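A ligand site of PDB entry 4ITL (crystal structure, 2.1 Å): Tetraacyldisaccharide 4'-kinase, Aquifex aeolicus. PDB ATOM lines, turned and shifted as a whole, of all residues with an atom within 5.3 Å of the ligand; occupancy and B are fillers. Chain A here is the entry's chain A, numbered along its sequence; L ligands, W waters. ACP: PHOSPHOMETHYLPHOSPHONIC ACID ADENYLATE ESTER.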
ATOM      1  N   ASN A  43       0.317 -23.196  23.233  1.00  0.00           N
ATOM      2  CA  ASN A  43       0.289 -24.644  23.297  1.00  0.00           C
ATOM      3  C   ASN A  43       0.747 -25.083  24.684  1.00  0.00           C
ATOM      4  O   ASN A  43       0.999 -24.235  25.557  1.00  0.00           O
ATOM      5  CB  ASN A  43       1.113 -25.280  22.155  1.00  0.00           C
ATOM      6  CG  ASN A  43       2.587 -25.257  22.414  1.00  0.00           C
ATOM      7  OD1 ASN A  43       3.146 -24.213  22.750  1.00  0.00           O
ATOM      8  ND2 ASN A  43       3.215 -26.423  22.320  1.00  0.00           N
ATOM      9  N   GLY A  47       8.836 -27.847  22.069  1.00  0.00           N
ATOM     10  CA  GLY A  47       9.155 -28.713  20.942  1.00  0.00           C
ATOM     11  C   GLY A  47       8.374 -28.373  19.674  1.00  0.00           C
ATOM     12  O   GLY A  47       8.479 -29.058  18.657  1.00  0.00           O
ATOM     13  N   GLY A  48       7.508 -27.383  19.759  1.00  0.00           N
ATOM     14  CA  GLY A  48       6.852 -26.846  18.574  1.00  0.00           C
ATOM     15  C   GLY A  48       5.504 -27.484  18.334  1.00  0.00           C
ATOM     16  O   GLY A  48       5.365 -28.697  18.412  1.00  0.00           O
ATOM     17  N   SER A  49       4.497 -26.661  18.054  1.00  0.00           N
ATOM     18  CA  SER A  49       3.162 -27.162  17.775  1.00  0.00           C
ATOM     19  C   SER A  49       2.466 -26.508  16.581  1.00  0.00           C
ATOM     20  O   SER A  49       1.253 -26.579  16.489  1.00  0.00           O
ATOM     21  CB  SER A  49       2.277 -27.012  19.012  1.00  0.00           C
ATOM     22  OG  SER A  49       2.168 -25.657  19.363  1.00  0.00           O
ATOM     23  N   GLY A  50       3.221 -25.878  15.694  1.00  0.00           N
ATOM     24  CA  GLY A  50       2.625 -25.113  14.615  1.00  0.00           C
ATOM     25  C   GLY A  50       1.932 -23.822  14.988  1.00  0.00           C
ATOM     26  O   GLY A  50       1.018 -23.379  14.301  1.00  0.00           O
ATOM     27  N   LYS A  51       2.367 -23.210  16.069  1.00  0.00           N
ATOM     28  CA  LYS A  51       1.805 -21.944  16.507  1.00  0.00           C
ATOM     29  C   LYS A  51       2.061 -20.819  15.522  1.00  0.00           C
ATOM     30  O   LYS A  51       1.145 -20.011  15.227  1.00  0.00           O
ATOM     31  CB  LYS A  51       2.409 -21.527  17.843  1.00  0.00           C
ATOM     32  CG  LYS A  51       1.829 -22.156  19.100  1.00  0.00           C
ATOM     33  CD  LYS A  51       2.697 -21.776  20.305  1.00  0.00           C
ATOM     34  CE  LYS A  51       4.024 -22.577  20.226  1.00  0.00           C
ATOM     35  NZ  LYS A  51       4.998 -22.172  21.225  1.00  0.00           N
ATOM     36  N   THR A  52       3.302 -20.689  15.062  1.00  0.00           N
ATOM     37  CA  THR A  52       3.617 -19.631  14.110  1.00  0.00           C
ATOM     38  C   THR A  52       2.745 -19.723  12.864  1.00  0.00           C
ATOM     39  O   THR A  52       2.209 -18.719  12.383  1.00  0.00           O
ATOM     40  CB  THR A  52       5.088 -19.670  13.709  1.00  0.00           C
ATOM     41  OG1 THR A  52       5.372 -20.967  13.213  1.00  0.00           O
ATOM     42  CG2 THR A  52       5.974 -19.401  14.883  1.00  0.00           C
ATOM     43  N   SER A  53       2.605 -20.931  12.338  1.00  0.00           N
ATOM     44  CA  SER A  53       1.775 -21.184  11.190  1.00  0.00           C
ATOM     45  C   SER A  53       0.324 -20.825  11.393  1.00  0.00           C
ATOM     46  O   SER A  53      -0.342 -20.254  10.504  1.00  0.00           O
ATOM     47  CB  SER A  53       1.872 -22.663  10.872  1.00  0.00           C
ATOM     48  OG  SER A  53       3.239 -22.973  10.644  1.00  0.00           O
ATOM     49  N   MET A  56      -0.048 -17.065  11.445  1.00  0.00           N
ATOM     50  CA  MET A  56      -0.094 -16.516  10.091  1.00  0.00           C
ATOM     51  C   MET A  56      -1.465 -16.737   9.423  1.00  0.00           C
ATOM     52  O   MET A  56      -1.999 -15.869   8.696  1.00  0.00           O
ATOM     53  CB  MET A  56       1.029 -17.114   9.233  1.00  0.00           C
ATOM     54  CG  MET A  56       2.423 -16.722   9.720  1.00  0.00           C
ATOM     55  SD  MET A  56       3.697 -17.633   8.825  1.00  0.00           S
ATOM     56  CE  MET A  56       5.206 -17.172   9.650  1.00  0.00           C
ATOM     57  N   GLU A 100      11.685 -16.135  14.998  1.00  0.00           N
ATOM     58  CA  GLU A 100      10.239 -16.277  14.756  1.00  0.00           C
ATOM     59  C   GLU A 100       9.471 -14.956  14.582  1.00  0.00           C
ATOM     60  O   GLU A 100       8.657 -14.818  13.670  1.00  0.00           O
ATOM     61  CB  GLU A 100       9.566 -17.213  15.789  1.00  0.00           C
ATOM     62  CG  GLU A 100      10.165 -18.650  15.669  1.00  0.00           C
ATOM     63  CD  GLU A 100       9.776 -19.587  16.807  1.00  0.00           C
ATOM     64  OE1 GLU A 100       8.979 -19.190  17.658  1.00  0.00           O
ATOM     65  OE2 GLU A 100      10.253 -20.751  16.840  1.00  0.00           O
ATOM     66  N   LEU A 103      10.341 -13.916  11.092  1.00  0.00           N
ATOM     67  CA  LEU A 103       9.755 -14.811  10.073  1.00  0.00           C
ATOM     68  C   LEU A 103       8.293 -14.412   9.839  1.00  0.00           C
ATOM     69  O   LEU A 103       7.824 -14.236   8.689  1.00  0.00           O
ATOM     70  CB  LEU A 103       9.847 -16.250  10.548  1.00  0.00           C
ATOM     71  CG  LEU A 103       9.019 -17.303   9.763  1.00  0.00           C
ATOM     72  CD1 LEU A 103       9.690 -17.582   8.455  1.00  0.00           C
ATOM     73  CD2 LEU A 103       8.821 -18.588  10.574  1.00  0.00           C
ATOM     74  N   TYR A 187      -0.639 -30.668  13.229  1.00  0.00           N
ATOM     75  CA  TYR A 187       0.173 -31.660  12.550  1.00  0.00           C
ATOM     76  C   TYR A 187      -0.626 -32.823  12.046  1.00  0.00           C
ATOM     77  O   TYR A 187      -0.115 -33.951  12.028  1.00  0.00           O
ATOM     78  CB  TYR A 187       1.290 -32.181  13.449  1.00  0.00           C
ATOM     79  CG  TYR A 187       2.299 -31.141  13.863  1.00  0.00           C
ATOM     80  CD1 TYR A 187       2.362 -29.897  13.238  1.00  0.00           C
ATOM     81  CD2 TYR A 187       3.185 -31.399  14.895  1.00  0.00           C
ATOM     82  CE1 TYR A 187       3.298 -28.966  13.627  1.00  0.00           C
ATOM     83  CE2 TYR A 187       4.115 -30.476  15.298  1.00  0.00           C
ATOM     84  CZ  TYR A 187       4.182 -29.249  14.672  1.00  0.00           C
ATOM     85  OH  TYR A 187       5.149 -28.333  15.100  1.00  0.00           O
ATOM     86  N   ARG A 206      -1.162 -28.888   7.307  1.00  0.00           N
ATOM     87  CA  ARG A 206      -0.184 -28.165   6.516  1.00  0.00           C
ATOM     88  C   ARG A 206      -0.128 -28.803   5.151  1.00  0.00           C
ATOM     89  O   ARG A 206       0.184 -30.005   5.030  1.00  0.00           O
ATOM     90  CB  ARG A 206       1.179 -28.178   7.201  1.00  0.00           C
ATOM     91  CG  ARG A 206       1.177 -27.373   8.497  1.00  0.00           C
ATOM     92  CD  ARG A 206       2.513 -27.402   9.225  1.00  0.00           C
ATOM     93  NE  ARG A 206       2.886 -28.785   9.505  1.00  0.00           N
ATOM     94  CZ  ARG A 206       4.066 -29.145   9.985  1.00  0.00           C
ATOM     95  NH1 ARG A 206       4.973 -28.228  10.276  1.00  0.00           N
ATOM     96  NH2 ARG A 206       4.338 -30.421  10.174  1.00  0.00           N
ATOM     97  N   PHE A 208       1.769 -29.052   1.945  1.00  0.00           N
ATOM     98  CA  PHE A 208       3.093 -28.767   1.426  1.00  0.00           C
ATOM     99  C   PHE A 208       3.044 -28.673  -0.071  1.00  0.00           C
ATOM    100  O   PHE A 208       2.952 -29.667  -0.733  1.00  0.00           O
ATOM    101  CB  PHE A 208       4.040 -29.874   1.873  1.00  0.00           C
ATOM    102  CG  PHE A 208       4.280 -29.844   3.315  1.00  0.00           C
ATOM    103  CD1 PHE A 208       3.574 -30.679   4.160  1.00  0.00           C
ATOM    104  CD2 PHE A 208       5.145 -28.889   3.854  1.00  0.00           C
ATOM    105  CE1 PHE A 208       3.748 -30.602   5.525  1.00  0.00           C
ATOM    106  CE2 PHE A 208       5.326 -28.805   5.220  1.00  0.00           C
ATOM    107  CZ  PHE A 208       4.622 -29.670   6.069  1.00  0.00           C
ATOM    108  N   LEU A 235      14.880 -26.546  14.649  1.00  0.00           N
ATOM    109  CA  LEU A 235      13.449 -26.489  14.884  1.00  0.00           C
ATOM    110  C   LEU A 235      13.194 -26.995  16.281  1.00  0.00           C
ATOM    111  O   LEU A 235      14.046 -27.638  16.872  1.00  0.00           O
ATOM    112  CB  LEU A 235      12.684 -27.342  13.889  1.00  0.00           C
ATOM    113  CG  LEU A 235      12.691 -26.908  12.436  1.00  0.00           C
ATOM    114  CD1 LEU A 235      11.765 -27.792  11.644  1.00  0.00           C
ATOM    115  CD2 LEU A 235      12.304 -25.446  12.285  1.00  0.00           C
ATOM    116  N   GLY A 236      12.019 -26.699  16.834  1.00  0.00           N
ATOM    117  CA  GLY A 236      11.634 -27.370  18.050  1.00  0.00           C
ATOM    118  C   GLY A 236      11.690 -28.880  17.904  1.00  0.00           C
ATOM    119  O   GLY A 236      12.125 -29.592  18.809  1.00  0.00           O
ATOM    120  N   ASP A 237      11.218 -29.377  16.765  1.00  0.00           N
ATOM    121  CA  ASP A 237      11.367 -30.809  16.453  1.00  0.00           C
ATOM    122  C   ASP A 237      11.693 -31.125  15.000  1.00  0.00           C
ATOM    123  O   ASP A 237      10.791 -31.178  14.136  1.00  0.00           O
ATOM    124  CB  ASP A 237      10.099 -31.536  16.819  1.00  0.00           C
ATOM    125  CG  ASP A 237      10.204 -33.023  16.535  1.00  0.00           C
ATOM    126  OD1 ASP A 237      11.343 -33.518  16.361  1.00  0.00           O
ATOM    127  OD2 ASP A 237       9.134 -33.686  16.499  1.00  0.00           O
ATOM    128  N   GLN A 240       9.774 -34.017  12.734  1.00  0.00           N
ATOM    129  CA  GLN A 240       8.559 -33.935  11.921  1.00  0.00           C
ATOM    130  C   GLN A 240       8.873 -33.415  10.513  1.00  0.00           C
ATOM    131  O   GLN A 240       8.223 -33.805   9.532  1.00  0.00           O
ATOM    132  CB  GLN A 240       7.382 -33.164  12.591  1.00  0.00           C
ATOM    133  CG  GLN A 240       7.691 -31.812  13.114  1.00  0.00           C
ATOM    134  CD  GLN A 240       7.728 -30.745  12.043  1.00  0.00           C
ATOM    135  OE1 GLN A 240       6.971 -30.794  11.048  1.00  0.00           O
ATOM    136  NE2 GLN A 240       8.621 -29.774  12.233  1.00  0.00           N
ATOM    137  N   PHE A 241       9.899 -32.577  10.418  1.00  0.00           N
ATOM    138  CA  PHE A 241      10.315 -32.069   9.115  1.00  0.00           C
ATOM    139  C   PHE A 241      10.874 -33.196   8.283  1.00  0.00           C
ATOM    140  O   PHE A 241      10.487 -33.350   7.114  1.00  0.00           O
ATOM    141  CB  PHE A 241      11.346 -30.939   9.264  1.00  0.00           C
ATOM    142  CG  PHE A 241      11.866 -30.432   7.959  1.00  0.00           C
ATOM    143  CD1 PHE A 241      10.999 -30.043   6.958  1.00  0.00           C
ATOM    144  CD2 PHE A 241      13.229 -30.266   7.769  1.00  0.00           C
ATOM    145  CE1 PHE A 241      11.493 -29.539   5.755  1.00  0.00           C
ATOM    146  CE2 PHE A 241      13.730 -29.755   6.566  1.00  0.00           C
ATOM    147  CZ  PHE A 241      12.855 -29.385   5.571  1.00  0.00           C
ATOM    148  N   VAL A 244       7.987 -35.348   7.108  1.00  0.00           N
ATOM    149  CA  VAL A 244       7.283 -34.688   6.008  1.00  0.00           C
ATOM    150  C   VAL A 244       8.018 -34.930   4.655  1.00  0.00           C
ATOM    151  O   VAL A 244       7.398 -35.294   3.652  1.00  0.00           O
ATOM    152  CB  VAL A 244       7.087 -33.173   6.287  1.00  0.00           C
ATOM    153  CG1 VAL A 244       6.729 -32.366   5.007  1.00  0.00           C
ATOM    154  CG2 VAL A 244       6.019 -32.950   7.402  1.00  0.00           C
ATOM    155  N   ASP A 260      17.313 -25.965  17.835  1.00  0.00           N
ATOM    156  CA  ASP A 260      16.295 -24.930  17.666  1.00  0.00           C
ATOM    157  C   ASP A 260      16.923 -23.527  17.648  1.00  0.00           C
ATOM    158  O   ASP A 260      17.885 -23.257  18.367  1.00  0.00           O
ATOM    159  CB  ASP A 260      15.239 -25.029  18.769  1.00  0.00           C
ATOM    160  CG  ASP A 260      13.930 -24.296  18.372  1.00  0.00           C
ATOM    161  OD1 ASP A 260      13.805 -23.784  17.220  1.00  0.00           O
ATOM    162  OD2 ASP A 260      13.008 -24.245  19.205  1.00  0.00           O
ATOM    163  N   HIS A 261      16.427 -22.665  16.768  1.00  0.00           N
ATOM    164  CA  HIS A 261      16.903 -21.272  16.627  1.00  0.00           C
ATOM    165  C   HIS A 261      18.386 -21.146  16.274  1.00  0.00           C
ATOM    166  O   HIS A 261      18.968 -20.095  16.467  1.00  0.00           O
ATOM    167  CB  HIS A 261      16.601 -20.464  17.897  1.00  0.00           C
ATOM    168  CG  HIS A 261      15.193 -20.591  18.372  1.00  0.00           C
ATOM    169  ND1 HIS A 261      14.125 -20.061  17.675  1.00  0.00           N
ATOM    170  CD2 HIS A 261      14.664 -21.197  19.455  1.00  0.00           C
ATOM    171  CE1 HIS A 261      13.003 -20.314  18.323  1.00  0.00           C
ATOM    172  NE2 HIS A 261      13.304 -21.014  19.410  1.00  0.00           N
ATOM    173  N   THR A 278      13.736 -25.159   5.950  1.00  0.00           N
ATOM    174  CA  THR A 278      12.426 -24.590   6.201  1.00  0.00           C
ATOM    175  C   THR A 278      12.509 -23.069   6.131  1.00  0.00           C
ATOM    176  O   THR A 278      13.585 -22.495   6.167  1.00  0.00           O
ATOM    177  CB  THR A 278      11.839 -24.983   7.584  1.00  0.00           C
ATOM    178  OG1 THR A 278      12.425 -24.197   8.624  1.00  0.00           O
ATOM    179  CG2 THR A 278      12.077 -26.446   7.904  1.00  0.00           C
ATOM    180  N   PRO A 279      11.356 -22.398   6.050  1.00  0.00           N
ATOM    181  CA  PRO A 279      11.445 -20.938   6.003  1.00  0.00           C
ATOM    182  C   PRO A 279      12.086 -20.297   7.254  1.00  0.00           C
ATOM    183  O   PRO A 279      12.745 -19.247   7.149  1.00  0.00           O
ATOM    184  CB  PRO A 279       9.982 -20.525   5.863  1.00  0.00           C
ATOM    185  CG  PRO A 279       9.371 -21.641   5.112  1.00  0.00           C
ATOM    186  CD  PRO A 279      10.011 -22.876   5.702  1.00  0.00           C
ATOM    187  N   LYS A 280      11.852 -20.888   8.415  1.00  0.00           N
ATOM    188  CA  LYS A 280      12.422 -20.455   9.684  1.00  0.00           C
ATOM    189  C   LYS A 280      13.918 -20.477   9.596  1.00  0.00           C
ATOM    190  O   LYS A 280      14.592 -19.565  10.083  1.00  0.00           O
ATOM    191  CB  LYS A 280      11.895 -21.347  10.844  1.00  0.00           C
ATOM    192  CG  LYS A 280      12.603 -21.201  12.143  1.00  0.00           C
ATOM    193  CD  LYS A 280      11.863 -21.886  13.259  1.00  0.00           C
ATOM    194  CE  LYS A 280      12.791 -22.061  14.450  1.00  0.00           C
ATOM    195  NZ  LYS A 280      12.030 -22.429  15.679  1.00  0.00           N
ATOM    196  N   LEU A 294      11.159 -25.698   1.825  1.00  0.00           N
ATOM    197  CA  LEU A 294       9.813 -26.216   1.637  1.00  0.00           C
ATOM    198  C   LEU A 294       8.803 -25.300   2.355  1.00  0.00           C
ATOM    199  O   LEU A 294       8.960 -24.977   3.528  1.00  0.00           O
ATOM    200  CB  LEU A 294       9.731 -27.619   2.208  1.00  0.00           C
ATOM    201  CG  LEU A 294       8.426 -28.391   2.040  1.00  0.00           C
ATOM    202  CD1 LEU A 294       8.186 -28.786   0.562  1.00  0.00           C
ATOM    203  CD2 LEU A 294       8.473 -29.628   2.905  1.00  0.00           C
ATOM    204  N   ASN A 295       7.779 -24.865   1.633  1.00  0.00           N
ATOM    205  CA  ASN A 295       6.735 -24.026   2.205  1.00  0.00           C
ATOM    206  C   ASN A 295       5.387 -24.718   2.032  1.00  0.00           C
ATOM    207  O   ASN A 295       5.218 -25.642   1.210  1.00  0.00           O
ATOM    208  CB  ASN A 295       6.713 -22.677   1.524  1.00  0.00           C
ATOM    209  CG  ASN A 295       6.057 -21.612   2.345  1.00  0.00           C
ATOM    210  OD1 ASN A 295       5.936 -21.711   3.579  1.00  0.00           O
ATOM    211  ND2 ASN A 295       5.667 -20.550   1.664  1.00  0.00           N
ATOM    212  N   PHE A 296       4.425 -24.253   2.787  1.00  0.00           N
ATOM    213  CA  PHE A 296       3.123 -24.893   2.857  1.00  0.00           C
ATOM    214  C   PHE A 296       2.022 -23.879   3.084  1.00  0.00           C
ATOM    215  O   PHE A 296       2.281 -22.779   3.585  1.00  0.00           O
ATOM    216  CB  PHE A 296       3.093 -25.914   4.009  1.00  0.00           C
ATOM    217  CG  PHE A 296       3.518 -25.334   5.344  1.00  0.00           C
ATOM    218  CD1 PHE A 296       2.576 -24.874   6.255  1.00  0.00           C
ATOM    219  CD2 PHE A 296       4.865 -25.264   5.681  1.00  0.00           C
ATOM    220  CE1 PHE A 296       2.970 -24.320   7.484  1.00  0.00           C
ATOM    221  CE2 PHE A 296       5.257 -24.722   6.903  1.00  0.00           C
ATOM    222  CZ  PHE A 296       4.316 -24.249   7.807  1.00  0.00           C
HETATM  223  PG  ACP L   1       7.922 -22.697  18.760  1.00  0.00           P
HETATM  224  O1G ACP L   1       8.834 -21.569  19.210  1.00  0.00           O
HETATM  225  O2G ACP L   1       7.035 -23.261  19.891  1.00  0.00           O
HETATM  226  O3G ACP L   1       8.821 -23.850  18.232  1.00  0.00           O
HETATM  227  PB  ACP L   1       6.099 -23.242  16.389  1.00  0.00           P
HETATM  228  O1B ACP L   1       5.281 -22.451  15.394  1.00  0.00           O
HETATM  229  O2B ACP L   1       5.093 -23.980  17.273  1.00  0.00           O
HETATM  230  C3B ACP L   1       6.919 -21.952  17.400  1.00  0.00           C
HETATM  231  PA  ACP L   1       6.977 -25.057  14.436  1.00  0.00           P
HETATM  232  O1A ACP L   1       5.798 -25.957  14.155  1.00  0.00           O
HETATM  233  O2A ACP L   1       8.292 -25.754  14.473  1.00  0.00           O
HETATM  234  O3A ACP L   1       7.019 -24.428  15.928  1.00  0.00           O
HETATM  235  O5' ACP L   1       6.994 -23.918  13.316  1.00  0.00           O
HETATM  236  C5' ACP L   1       8.130 -23.059  13.249  1.00  0.00           C
HETATM  237  C4' ACP L   1       8.420 -22.665  11.805  1.00  0.00           C
HETATM  238  O4' ACP L   1       9.366 -23.631  11.345  1.00  0.00           O
HETATM  239  C3' ACP L   1       7.292 -22.715  10.832  1.00  0.00           C
HETATM  240  O3' ACP L   1       6.569 -21.569  10.740  1.00  0.00           O
HETATM  241  C2' ACP L   1       8.004 -23.018   9.562  1.00  0.00           C
HETATM  242  O2' ACP L   1       8.632 -21.936   8.935  1.00  0.00           O
HETATM  243  C1' ACP L   1       9.031 -23.969  10.036  1.00  0.00           C
HETATM  244  N9  ACP L   1       8.656 -25.371   9.948  1.00  0.00           N
HETATM  245  C8  ACP L   1       8.434 -26.243  10.971  1.00  0.00           C
HETATM  246  N7  ACP L   1       8.126 -27.447  10.459  1.00  0.00           N
HETATM  247  C5  ACP L   1       8.176 -27.377   9.122  1.00  0.00           C
HETATM  248  C6  ACP L   1       7.961 -28.285   8.085  1.00  0.00           C
HETATM  249  N6  ACP L   1       7.596 -29.645   8.377  1.00  0.00           N
HETATM  250  N1  ACP L   1       8.064 -27.872   6.815  1.00  0.00           N
HETATM  251  C2  ACP L   1       8.382 -26.591   6.499  1.00  0.00           C
HETATM  252  N3  ACP L   1       8.604 -25.676   7.472  1.00  0.00           N
HETATM  253  C4  ACP L   1       8.502 -26.050   8.774  1.00  0.00           C
HETATM  254  O   HOH W   1       4.554 -25.621  11.400  1.00  0.00           O
HETATM  255  O   HOH W   2       9.367 -28.264  14.976  1.00  0.00           O
HETATM  256  O   HOH W   3       6.891 -20.590   7.917  1.00  0.00           O
HETATM  257  O   HOH W   4      11.247 -21.977  21.109  1.00  0.00           O
HETATM  258  O   HOH W   5       6.584 -25.389  21.601  1.00  0.00           O
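Water W5 lies within hydrogen-bond range of O2G of the ligand (2.8 Å), N of Gly 48 (2.9 Å) and N of Gly 47 (3.4 Å). Water W2 lies within hydrogen-bond range of O2A of the ligand (2.8 Å), N of Asp 237 (2.8 Å) and NE2 of Gln 240 (3.2 Å). Water W1 lies within hydrogen-bond range of NH1 of Arg 206 (2.9 Å), O1A of the ligand (3.0 Å) and OG of Ser 53 (3.1 Å). Water W4 lies within hydrogen-bond range of NE2 of His 261, O1G of the ligand and OD2 of Asp 260.
OG1 of Thr 278 sits close to N of Lys 280 (3.4 Å). The side-chain hydroxyl (OH) of Tyr 187 is in hydrogen-bond range of the backbone carbonyl oxygen (O) of Gly 48. The side-chain amide oxygen (OE1) of Gln 240 sits at hydrogen-bond distance from the guanidinium group (NH2) of Arg 206 (2.8 Å). OG of Ser 49 lies close to ND2 of Asn 43 (3.2 Å). NZ of Lys 51 lies close to OD1 of Asn 43 (3.1 Å). The backbone carbonyl oxygen (O) of Asp 237 lies within hydrogen-bond range of the side-chain amide nitrogen (NE2) of Gln 240 (3.2 Å). The backbone NH of Gly 50 is in hydrogen-bond range of the side-chain hydroxyl of Tyr 187 (3.2 Å). The backbone NH (N) of Ser 49 lies within hydrogen-bond range of the side-chain hydroxyl (OH) of Tyr 187 (3.5 Å).
N of Gly 50 lies within hydrogen-bond range of O1A of the ligand (3.0 Å). An oxygen (O1G) of the ligand sits close to the side-chain carboxylate (OE1) of Glu 100. O2B of the ligand lies within hydrogen-bond range of N of Ser 49 (2.9 Å). O2' of the ligand lies within hydrogen-bond range of N of Lys 280 (3.4 Å). O2B of the ligand sits at hydrogen-bond distance from N of Lys 51. The side-chain hydroxyl of Tyr 187 sits at hydrogen-bond distance from an oxygen (O1A) of the ligand, 2.6 Å away. A nitrogen (N7) of the ligand lies within hydrogen-bond range of the side-chain amide nitrogen (NE2) of Gln 240 (3.0 Å). The backbone NH (N) of Thr 52 lies within hydrogen-bond range of an oxygen (O1B) of the ligand. The side-chain hydroxyl (OG1) of Thr 52 is in hydrogen-bond range of an oxygen (O1B) of the ligand (2.6 Å). The guanidinium group (NH1) of Arg 206 sits at hydrogen-bond distance from a nitrogen (N7) of the ligand, at 3.3 Å. O2G of the ligand lies within salt-bridge range of NZ of Lys 51 (2.7 Å).
Residues that only touch the ligand: Phe 208 (3.3 Å), Thr 278 (3.3 Å), Leu 294 (3.4 Å), Phe 296 (3.5 Å), Leu 235 (3.6 Å), Gly 48 (3.6 Å), Pro 279 (3.6 Å), Ser 53 (3.6 Å), Phe 241 (3.7 Å), Leu 103 (3.7 Å) and Val 244 (3.8 Å). Of the 28 residues printed, 20 come within 4 Å of the ligand.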
